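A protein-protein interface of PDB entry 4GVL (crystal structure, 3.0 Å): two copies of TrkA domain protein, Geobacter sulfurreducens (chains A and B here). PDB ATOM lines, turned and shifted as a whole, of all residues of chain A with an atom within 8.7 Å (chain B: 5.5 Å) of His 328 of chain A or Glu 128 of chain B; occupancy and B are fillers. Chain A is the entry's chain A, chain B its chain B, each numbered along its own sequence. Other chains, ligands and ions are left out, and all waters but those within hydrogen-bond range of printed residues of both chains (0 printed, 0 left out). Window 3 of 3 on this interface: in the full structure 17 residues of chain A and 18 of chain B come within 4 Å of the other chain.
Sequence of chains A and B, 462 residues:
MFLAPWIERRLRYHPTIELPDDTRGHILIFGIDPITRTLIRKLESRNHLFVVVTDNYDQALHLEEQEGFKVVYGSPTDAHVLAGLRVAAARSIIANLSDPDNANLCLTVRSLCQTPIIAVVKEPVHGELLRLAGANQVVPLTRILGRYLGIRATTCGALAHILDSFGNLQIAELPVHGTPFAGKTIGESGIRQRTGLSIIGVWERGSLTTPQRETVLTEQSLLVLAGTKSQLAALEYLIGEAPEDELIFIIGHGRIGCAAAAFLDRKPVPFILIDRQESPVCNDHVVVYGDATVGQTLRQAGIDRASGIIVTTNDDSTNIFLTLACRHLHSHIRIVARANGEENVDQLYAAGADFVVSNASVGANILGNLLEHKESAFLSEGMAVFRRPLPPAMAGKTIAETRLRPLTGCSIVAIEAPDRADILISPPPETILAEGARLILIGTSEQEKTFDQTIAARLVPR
No position is printed for both chains.
Of the 17 printed residues of chain A, 3 touch a printed residue of chain B. Hydrophobic or aromatic side chains of chain A that line the printed part of chain B: Phe 321, Leu 324 and His 328.
Printed residues of chain B within 4 Å of Phe 321 of chain A: His 126. Printed residues of chain B within 4 Å of Leu 324 of chain A: Leu 129 and Leu 132. Of chain B, only Glu 128 (2.8 Å), Leu 129 (3.6 Å) and Leu 132 (3.4 Å) come within 4 Å of His 328 of chain A. No residue of chain A comes within 4 Å of Gly 127 of chain B. Of the printed residues of chain A, Glu 128 of chain B touches His 328 (2.8 Å). Of the printed residues of chain A, Leu 129 of chain B touches Leu 324 and His 328. Printed residues of chain A within 4 Å of Leu 132 of chain B: Leu 324 (3.99 Å) and His 328 (3.4 Å). The nearest printed residue of chain B that does not touch His 328 of chain A is Val 125 of chain B (6.5 Å). The nearest residue of chain A that does not touch Glu 128 of chain B is Leu 329 of chain A (5.7 Å). The nearest printed residue of chain A that does not touch His 126 of chain B is Leu 324 of chain A (6.8 Å).
NE2 of His 126 of chain B touches CZ of Phe 321 of chain A, 3.5 Å away. Leu 324 of chain A touches Leu 129 of chain B. CB of Leu 132 of chain B touches CD2 of Leu 324 of chain A, at 3.99 Å. His 328 of chain A touches Leu 129 of chain B. ND1 of His 328 of chain A touches CD1 of Leu 132 of chain B, at 3.4 Å.
The side-chain carboxylate (OE2) of Glu 128 of chain B lies within hydrogen-bond range of a ring nitrogen (NE2) of His 328 of chain A, at 2.8 Å.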
ATOM      1  N   ARG A 299     -19.188 -13.782   2.223  1.00  0.00           N
ATOM      2  CA  ARG A 299     -18.245 -12.789   1.730  1.00  0.00           C
ATOM      3  C   ARG A 299     -18.070 -11.648   2.730  1.00  0.00           C
ATOM      4  O   ARG A 299     -16.954 -11.380   3.182  1.00  0.00           O
ATOM      5  CB  ARG A 299     -18.691 -12.245   0.372  1.00  0.00           C
ATOM      6  CG  ARG A 299     -17.529 -11.901  -0.561  1.00  0.00           C
ATOM      7  CD  ARG A 299     -17.866 -12.209  -2.022  1.00  0.00           C
ATOM      8  NE  ARG A 299     -18.990 -13.149  -2.147  1.00  0.00           N
ATOM      9  CZ  ARG A 299     -19.102 -14.109  -3.068  1.00  0.00           C
ATOM     10  NH1 ARG A 299     -18.142 -14.309  -3.968  1.00  0.00           N
ATOM     11  NH2 ARG A 299     -20.182 -14.886  -3.073  1.00  0.00           N
ATOM     12  N   PHE A 321     -23.977 -28.332  -0.256  1.00  0.00           N
ATOM     13  CA  PHE A 321     -24.070 -27.084  -0.989  1.00  0.00           C
ATOM     14  C   PHE A 321     -22.931 -26.115  -0.639  1.00  0.00           C
ATOM     15  O   PHE A 321     -22.410 -25.407  -1.506  1.00  0.00           O
ATOM     16  CB  PHE A 321     -25.417 -26.445  -0.705  1.00  0.00           C
ATOM     17  CG  PHE A 321     -25.685 -25.241  -1.514  1.00  0.00           C
ATOM     18  CD1 PHE A 321     -26.242 -25.361  -2.779  1.00  0.00           C
ATOM     19  CD2 PHE A 321     -25.382 -23.977  -1.017  1.00  0.00           C
ATOM     20  CE1 PHE A 321     -26.496 -24.228  -3.554  1.00  0.00           C
ATOM     21  CE2 PHE A 321     -25.624 -22.836  -1.768  1.00  0.00           C
ATOM     22  CZ  PHE A 321     -26.184 -22.957  -3.043  1.00  0.00           C
ATOM     23  N   LEU A 322     -22.540 -26.098   0.634  1.00  0.00           N
ATOM     24  CA  LEU A 322     -21.605 -25.090   1.118  1.00  0.00           C
ATOM     25  C   LEU A 322     -20.178 -25.440   0.735  1.00  0.00           C
ATOM     26  O   LEU A 322     -19.360 -24.552   0.428  1.00  0.00           O
ATOM     27  CB  LEU A 322     -21.741 -24.929   2.625  1.00  0.00           C
ATOM     28  CG  LEU A 322     -22.933 -24.087   3.061  1.00  0.00           C
ATOM     29  CD1 LEU A 322     -22.981 -24.031   4.574  1.00  0.00           C
ATOM     30  CD2 LEU A 322     -22.896 -22.677   2.449  1.00  0.00           C
ATOM     31  N   THR A 323     -19.900 -26.743   0.759  1.00  0.00           N
ATOM     32  CA  THR A 323     -18.611 -27.266   0.350  1.00  0.00           C
ATOM     33  C   THR A 323     -18.405 -26.973  -1.131  1.00  0.00           C
ATOM     34  O   THR A 323     -17.377 -26.410  -1.498  1.00  0.00           O
ATOM     35  CB  THR A 323     -18.509 -28.785   0.601  1.00  0.00           C
ATOM     36  OG1 THR A 323     -18.776 -29.077   1.984  1.00  0.00           O
ATOM     37  CG2 THR A 323     -17.131 -29.303   0.212  1.00  0.00           C
ATOM     38  N   LEU A 324     -19.381 -27.345  -1.969  1.00  0.00           N
ATOM     39  CA  LEU A 324     -19.343 -27.014  -3.393  1.00  0.00           C
ATOM     40  C   LEU A 324     -19.032 -25.547  -3.566  1.00  0.00           C
ATOM     41  O   LEU A 324     -18.094 -25.170  -4.279  1.00  0.00           O
ATOM     42  CB  LEU A 324     -20.695 -27.252  -4.040  1.00  0.00           C
ATOM     43  CG  LEU A 324     -21.059 -28.450  -4.898  1.00  0.00           C
ATOM     44  CD1 LEU A 324     -22.398 -28.121  -5.509  1.00  0.00           C
ATOM     45  CD2 LEU A 324     -20.025 -28.731  -5.974  1.00  0.00           C
ATOM     46  N   ALA A 325     -19.834 -24.727  -2.886  1.00  0.00           N
ATOM     47  CA  ALA A 325     -19.782 -23.285  -3.025  1.00  0.00           C
ATOM     48  C   ALA A 325     -18.381 -22.754  -2.753  1.00  0.00           C
ATOM     49  O   ALA A 325     -17.858 -21.958  -3.531  1.00  0.00           O
ATOM     50  CB  ALA A 325     -20.776 -22.658  -2.117  1.00  0.00           C
ATOM     51  N   CYS A 326     -17.765 -23.230  -1.673  1.00  0.00           N
ATOM     52  CA  CYS A 326     -16.435 -22.765  -1.276  1.00  0.00           C
ATOM     53  C   CYS A 326     -15.337 -23.325  -2.129  1.00  0.00           C
ATOM     54  O   CYS A 326     -14.419 -22.601  -2.507  1.00  0.00           O
ATOM     55  CB  CYS A 326     -16.140 -23.132   0.159  1.00  0.00           C
ATOM     56  SG  CYS A 326     -17.250 -22.326   1.254  1.00  0.00           S
ATOM     57  N   ARG A 327     -15.407 -24.620  -2.402  1.00  0.00           N
ATOM     58  CA  ARG A 327     -14.432 -25.221  -3.260  1.00  0.00           C
ATOM     59  C   ARG A 327     -14.458 -24.451  -4.568  1.00  0.00           C
ATOM     60  O   ARG A 327     -13.409 -24.186  -5.155  1.00  0.00           O
ATOM     61  CB  ARG A 327     -14.743 -26.691  -3.499  1.00  0.00           C
ATOM     62  CG  ARG A 327     -13.719 -27.390  -4.378  1.00  0.00           C
ATOM     63  CD  ARG A 327     -12.622 -28.023  -3.561  1.00  0.00           C
ATOM     64  NE  ARG A 327     -11.691 -27.063  -2.989  1.00  0.00           N
ATOM     65  CZ  ARG A 327     -11.196 -27.157  -1.758  1.00  0.00           C
ATOM     66  NH1 ARG A 327     -10.343 -26.245  -1.311  1.00  0.00           N
ATOM     67  NH2 ARG A 327     -11.563 -28.151  -0.967  1.00  0.00           N
ATOM     68  N   HIS A 328     -15.655 -24.064  -5.004  1.00  0.00           N
ATOM     69  CA  HIS A 328     -15.774 -23.367  -6.267  1.00  0.00           C
ATOM     70  C   HIS A 328     -15.168 -21.978  -6.228  1.00  0.00           C
ATOM     71  O   HIS A 328     -14.361 -21.637  -7.083  1.00  0.00           O
ATOM     72  CB  HIS A 328     -17.220 -23.286  -6.749  1.00  0.00           C
ATOM     73  CG  HIS A 328     -17.369 -22.565  -8.056  1.00  0.00           C
ATOM     74  ND1 HIS A 328     -16.837 -23.044  -9.235  1.00  0.00           N
ATOM     75  CD2 HIS A 328     -17.972 -21.392  -8.367  1.00  0.00           C
ATOM     76  CE1 HIS A 328     -17.113 -22.203 -10.214  1.00  0.00           C
ATOM     77  NE2 HIS A 328     -17.802 -21.194  -9.715  1.00  0.00           N
ATOM     78  N   LEU A 329     -15.553 -21.178  -5.242  1.00  0.00           N
ATOM     79  CA  LEU A 329     -15.181 -19.769  -5.260  1.00  0.00           C
ATOM     80  C   LEU A 329     -13.883 -19.424  -4.535  1.00  0.00           C
ATOM     81  O   LEU A 329     -13.292 -18.366  -4.781  1.00  0.00           O
ATOM     82  CB  LEU A 329     -16.347 -18.886  -4.808  1.00  0.00           C
ATOM     83  CG  LEU A 329     -17.435 -18.814  -5.892  1.00  0.00           C
ATOM     84  CD1 LEU A 329     -18.716 -19.521  -5.432  1.00  0.00           C
ATOM     85  CD2 LEU A 329     -17.721 -17.365  -6.317  1.00  0.00           C
ATOM     86  N   HIS A 330     -13.443 -20.319  -3.649  1.00  0.00           N
ATOM     87  CA  HIS A 330     -12.164 -20.175  -2.943  1.00  0.00           C
ATOM     88  C   HIS A 330     -11.471 -21.539  -2.931  1.00  0.00           C
ATOM     89  O   HIS A 330     -11.473 -22.250  -1.924  1.00  0.00           O
ATOM     90  CB  HIS A 330     -12.376 -19.601  -1.530  1.00  0.00           C
ATOM     91  CG  HIS A 330     -13.276 -18.397  -1.495  1.00  0.00           C
ATOM     92  ND1 HIS A 330     -14.571 -18.444  -1.013  1.00  0.00           N
ATOM     93  CD2 HIS A 330     -13.083 -17.124  -1.927  1.00  0.00           C
ATOM     94  CE1 HIS A 330     -15.128 -17.250  -1.134  1.00  0.00           C
ATOM     95  NE2 HIS A 330     -14.247 -16.431  -1.686  1.00  0.00           N
ATOM     96  N   SER A 331     -10.896 -21.898  -4.077  1.00  0.00           N
ATOM     97  CA  SER A 331     -10.360 -23.245  -4.320  1.00  0.00           C
ATOM     98  C   SER A 331      -9.168 -23.643  -3.442  1.00  0.00           C
ATOM     99  O   SER A 331      -9.028 -24.816  -3.077  1.00  0.00           O
ATOM    100  CB  SER A 331      -9.975 -23.398  -5.785  1.00  0.00           C
ATOM    101  OG  SER A 331      -8.999 -22.438  -6.129  1.00  0.00           O
ATOM    102  N   HIS A 332      -8.314 -22.669  -3.123  1.00  0.00           N
ATOM    103  CA  HIS A 332      -7.136 -22.885  -2.280  1.00  0.00           C
ATOM    104  C   HIS A 332      -7.501 -23.205  -0.818  1.00  0.00           C
ATOM    105  O   HIS A 332      -6.767 -23.930  -0.138  1.00  0.00           O
ATOM    106  CB  HIS A 332      -6.210 -21.666  -2.345  1.00  0.00           C
ATOM    107  CG  HIS A 332      -6.811 -20.417  -1.770  1.00  0.00           C
ATOM    108  ND1 HIS A 332      -7.819 -19.713  -2.398  1.00  0.00           N
ATOM    109  CD2 HIS A 332      -6.550 -19.749  -0.618  1.00  0.00           C
ATOM    110  CE1 HIS A 332      -8.150 -18.667  -1.661  1.00  0.00           C
ATOM    111  NE2 HIS A 332      -7.397 -18.666  -0.575  1.00  0.00           N
ATOM    112  N   ILE A 333      -8.635 -22.672  -0.359  1.00  0.00           N
ATOM    113  CA  ILE A 333      -9.084 -22.782   1.037  1.00  0.00           C
ATOM    114  C   ILE A 333      -9.424 -24.227   1.464  1.00  0.00           C
ATOM    115  O   ILE A 333     -10.257 -24.874   0.834  1.00  0.00           O
ATOM    116  CB  ILE A 333     -10.271 -21.783   1.307  1.00  0.00           C
ATOM    117  CG1 ILE A 333      -9.729 -20.337   1.390  1.00  0.00           C
ATOM    118  CG2 ILE A 333     -11.039 -22.136   2.574  1.00  0.00           C
ATOM    119  CD1 ILE A 333     -10.761 -19.184   1.155  1.00  0.00           C
ATOM    120  N   ILE A 335     -11.011 -27.377   3.506  1.00  0.00           N
ATOM    121  CA  ILE A 335     -12.408 -27.550   3.934  1.00  0.00           C
ATOM    122  C   ILE A 335     -12.689 -28.867   4.687  1.00  0.00           C
ATOM    123  O   ILE A 335     -12.608 -29.963   4.123  1.00  0.00           O
ATOM    124  CB  ILE A 335     -13.380 -27.468   2.727  1.00  0.00           C
ATOM    125  CG1 ILE A 335     -13.200 -26.173   1.951  1.00  0.00           C
ATOM    126  CG2 ILE A 335     -14.816 -27.578   3.172  1.00  0.00           C
ATOM    127  CD1 ILE A 335     -13.864 -26.180   0.571  1.00  0.00           C
ATOM    128  N   ALA A 351     -18.017 -33.202  -3.430  1.00  0.00           N
ATOM    129  CA  ALA A 351     -18.260 -31.774  -3.556  1.00  0.00           C
ATOM    130  C   ALA A 351     -16.975 -30.979  -3.459  1.00  0.00           C
ATOM    131  O   ALA A 351     -16.875 -29.895  -4.026  1.00  0.00           O
ATOM    132  CB  ALA A 351     -19.233 -31.319  -2.541  1.00  0.00           C
ATOM    133  N   GLY A 352     -15.983 -31.510  -2.755  1.00  0.00           N
ATOM    134  CA  GLY A 352     -14.685 -30.856  -2.711  1.00  0.00           C
ATOM    135  C   GLY A 352     -14.058 -30.779  -1.337  1.00  0.00           C
ATOM    136  O   GLY A 352     -13.014 -30.132  -1.162  1.00  0.00           O
ATOM    137  N   PRO B 124     -30.164 -17.800  -9.763  1.00  0.00           N
ATOM    138  CA  PRO B 124     -29.207 -17.572 -10.837  1.00  0.00           C
ATOM    139  C   PRO B 124     -27.769 -18.059 -10.577  1.00  0.00           C
ATOM    140  O   PRO B 124     -27.297 -18.945 -11.286  1.00  0.00           O
ATOM    141  CB  PRO B 124     -29.271 -16.052 -10.998  1.00  0.00           C
ATOM    142  CG  PRO B 124     -30.794 -15.739 -10.707  1.00  0.00           C
ATOM    143  CD  PRO B 124     -31.352 -16.942  -9.925  1.00  0.00           C
ATOM    144  N   VAL B 125     -27.099 -17.520  -9.567  1.00  0.00           N
ATOM    145  CA  VAL B 125     -25.688 -17.845  -9.312  1.00  0.00           C
ATOM    146  C   VAL B 125     -25.405 -19.318  -8.996  1.00  0.00           C
ATOM    147  O   VAL B 125     -24.274 -19.785  -9.130  1.00  0.00           O
ATOM    148  CB  VAL B 125     -25.123 -17.012  -8.162  1.00  0.00           C
ATOM    149  CG1 VAL B 125     -23.623 -16.754  -8.399  1.00  0.00           C
ATOM    150  CG2 VAL B 125     -25.900 -15.690  -8.017  1.00  0.00           C
ATOM    151  N   HIS B 126     -26.442 -20.035  -8.579  1.00  0.00           N
ATOM    152  CA  HIS B 126     -26.338 -21.445  -8.230  1.00  0.00           C
ATOM    153  C   HIS B 126     -26.202 -22.369  -9.428  1.00  0.00           C
ATOM    154  O   HIS B 126     -25.727 -23.488  -9.281  1.00  0.00           O
ATOM    155  CB  HIS B 126     -27.532 -21.877  -7.381  1.00  0.00           C
ATOM    156  CG  HIS B 126     -27.625 -21.158  -6.072  1.00  0.00           C
ATOM    157  ND1 HIS B 126     -28.708 -21.280  -5.231  1.00  0.00           N
ATOM    158  CD2 HIS B 126     -26.772 -20.292  -5.468  1.00  0.00           C
ATOM    159  CE1 HIS B 126     -28.513 -20.533  -4.159  1.00  0.00           C
ATOM    160  NE2 HIS B 126     -27.349 -19.918  -4.280  1.00  0.00           N
ATOM    161  N   GLY B 127     -26.620 -21.907 -10.605  1.00  0.00           N
ATOM    162  CA  GLY B 127     -26.514 -22.693 -11.836  1.00  0.00           C
ATOM    163  C   GLY B 127     -25.147 -23.312 -12.069  1.00  0.00           C
ATOM    164  O   GLY B 127     -25.040 -24.511 -12.335  1.00  0.00           O
ATOM    165  N   GLU B 128     -24.101 -22.494 -11.964  1.00  0.00           N
ATOM    166  CA  GLU B 128     -22.727 -22.986 -12.000  1.00  0.00           C
ATOM    167  C   GLU B 128     -22.550 -24.198 -11.091  1.00  0.00           C
ATOM    168  O   GLU B 128     -22.064 -25.242 -11.512  1.00  0.00           O
ATOM    169  CB  GLU B 128     -21.766 -21.900 -11.533  1.00  0.00           C
ATOM    170  CG  GLU B 128     -21.532 -20.780 -12.526  1.00  0.00           C
ATOM    171  CD  GLU B 128     -20.683 -19.655 -11.936  1.00  0.00           C
ATOM    172  OE1 GLU B 128     -20.765 -18.510 -12.448  1.00  0.00           O
ATOM    173  OE2 GLU B 128     -19.938 -19.908 -10.954  1.00  0.00           O
ATOM    174  N   LEU B 129     -22.956 -24.040  -9.840  1.00  0.00           N
ATOM    175  CA  LEU B 129     -22.800 -25.072  -8.837  1.00  0.00           C
ATOM    176  C   LEU B 129     -23.577 -26.357  -9.146  1.00  0.00           C
ATOM    177  O   LEU B 129     -23.086 -27.455  -8.916  1.00  0.00           O
ATOM    178  CB  LEU B 129     -23.186 -24.508  -7.467  1.00  0.00           C
ATOM    179  CG  LEU B 129     -22.156 -23.757  -6.605  1.00  0.00           C
ATOM    180  CD1 LEU B 129     -21.024 -23.082  -7.372  1.00  0.00           C
ATOM    181  CD2 LEU B 129     -22.874 -22.752  -5.736  1.00  0.00           C
ATOM    182  N   LEU B 130     -24.781 -26.227  -9.680  1.00  0.00           N
ATOM    183  CA  LEU B 130     -25.552 -27.409 -10.052  1.00  0.00           C
ATOM    184  C   LEU B 130     -24.943 -28.160 -11.243  1.00  0.00           C
ATOM    185  O   LEU B 130     -25.128 -29.371 -11.387  1.00  0.00           O
ATOM    186  CB  LEU B 130     -27.020 -27.052 -10.329  1.00  0.00           C
ATOM    187  CG  LEU B 130     -28.002 -26.935  -9.162  1.00  0.00           C
ATOM    188  CD1 LEU B 130     -27.944 -28.158  -8.269  1.00  0.00           C
ATOM    189  CD2 LEU B 130     -27.703 -25.699  -8.359  1.00  0.00           C
ATOM    190  N   ARG B 131     -24.233 -27.437 -12.102  1.00  0.00           N
ATOM    191  CA  ARG B 131     -23.448 -28.083 -13.142  1.00  0.00           C
ATOM    192  C   ARG B 131     -22.330 -28.891 -12.512  1.00  0.00           C
ATOM    193  O   ARG B 131     -22.213 -30.079 -12.790  1.00  0.00           O
ATOM    194  CB  ARG B 131     -22.880 -27.083 -14.147  1.00  0.00           C
ATOM    195  CG  ARG B 131     -23.872 -26.684 -15.194  1.00  0.00           C
ATOM    196  CD  ARG B 131     -23.205 -25.988 -16.370  1.00  0.00           C
ATOM    197  NE  ARG B 131     -24.187 -25.216 -17.130  1.00  0.00           N
ATOM    198  CZ  ARG B 131     -25.130 -25.745 -17.910  1.00  0.00           C
ATOM    199  NH1 ARG B 131     -25.235 -27.067 -18.056  1.00  0.00           N
ATOM    200  NH2 ARG B 131     -25.976 -24.944 -18.544  1.00  0.00           N
ATOM    201  N   LEU B 132     -21.525 -28.253 -11.661  1.00  0.00           N
ATOM    202  CA  LEU B 132     -20.466 -28.939 -10.939  1.00  0.00           C
ATOM    203  C   LEU B 132     -20.997 -30.195 -10.273  1.00  0.00           C
ATOM    204  O   LEU B 132     -20.356 -31.237 -10.313  1.00  0.00           O
ATOM    205  CB  LEU B 132     -19.835 -28.024  -9.898  1.00  0.00           C
ATOM    206  CG  LEU B 132     -18.701 -27.136 -10.403  1.00  0.00           C
ATOM    207  CD1 LEU B 132     -18.602 -25.873  -9.581  1.00  0.00           C
ATOM    208  CD2 LEU B 132     -17.359 -27.857 -10.426  1.00  0.00           C
ATOM    209  N   ALA B 133     -22.181 -30.104  -9.685  1.00  0.00           N
ATOM    210  CA  ALA B 133     -22.757 -31.245  -8.989  1.00  0.00           C
ATOM    211  C   ALA B 133     -23.209 -32.302  -9.974  1.00  0.00           C
ATOM    212  O   ALA B 133     -23.584 -33.408  -9.587  1.00  0.00           O
ATOM    213  CB  ALA B 133     -23.915 -30.810  -8.117  1.00  0.00           C
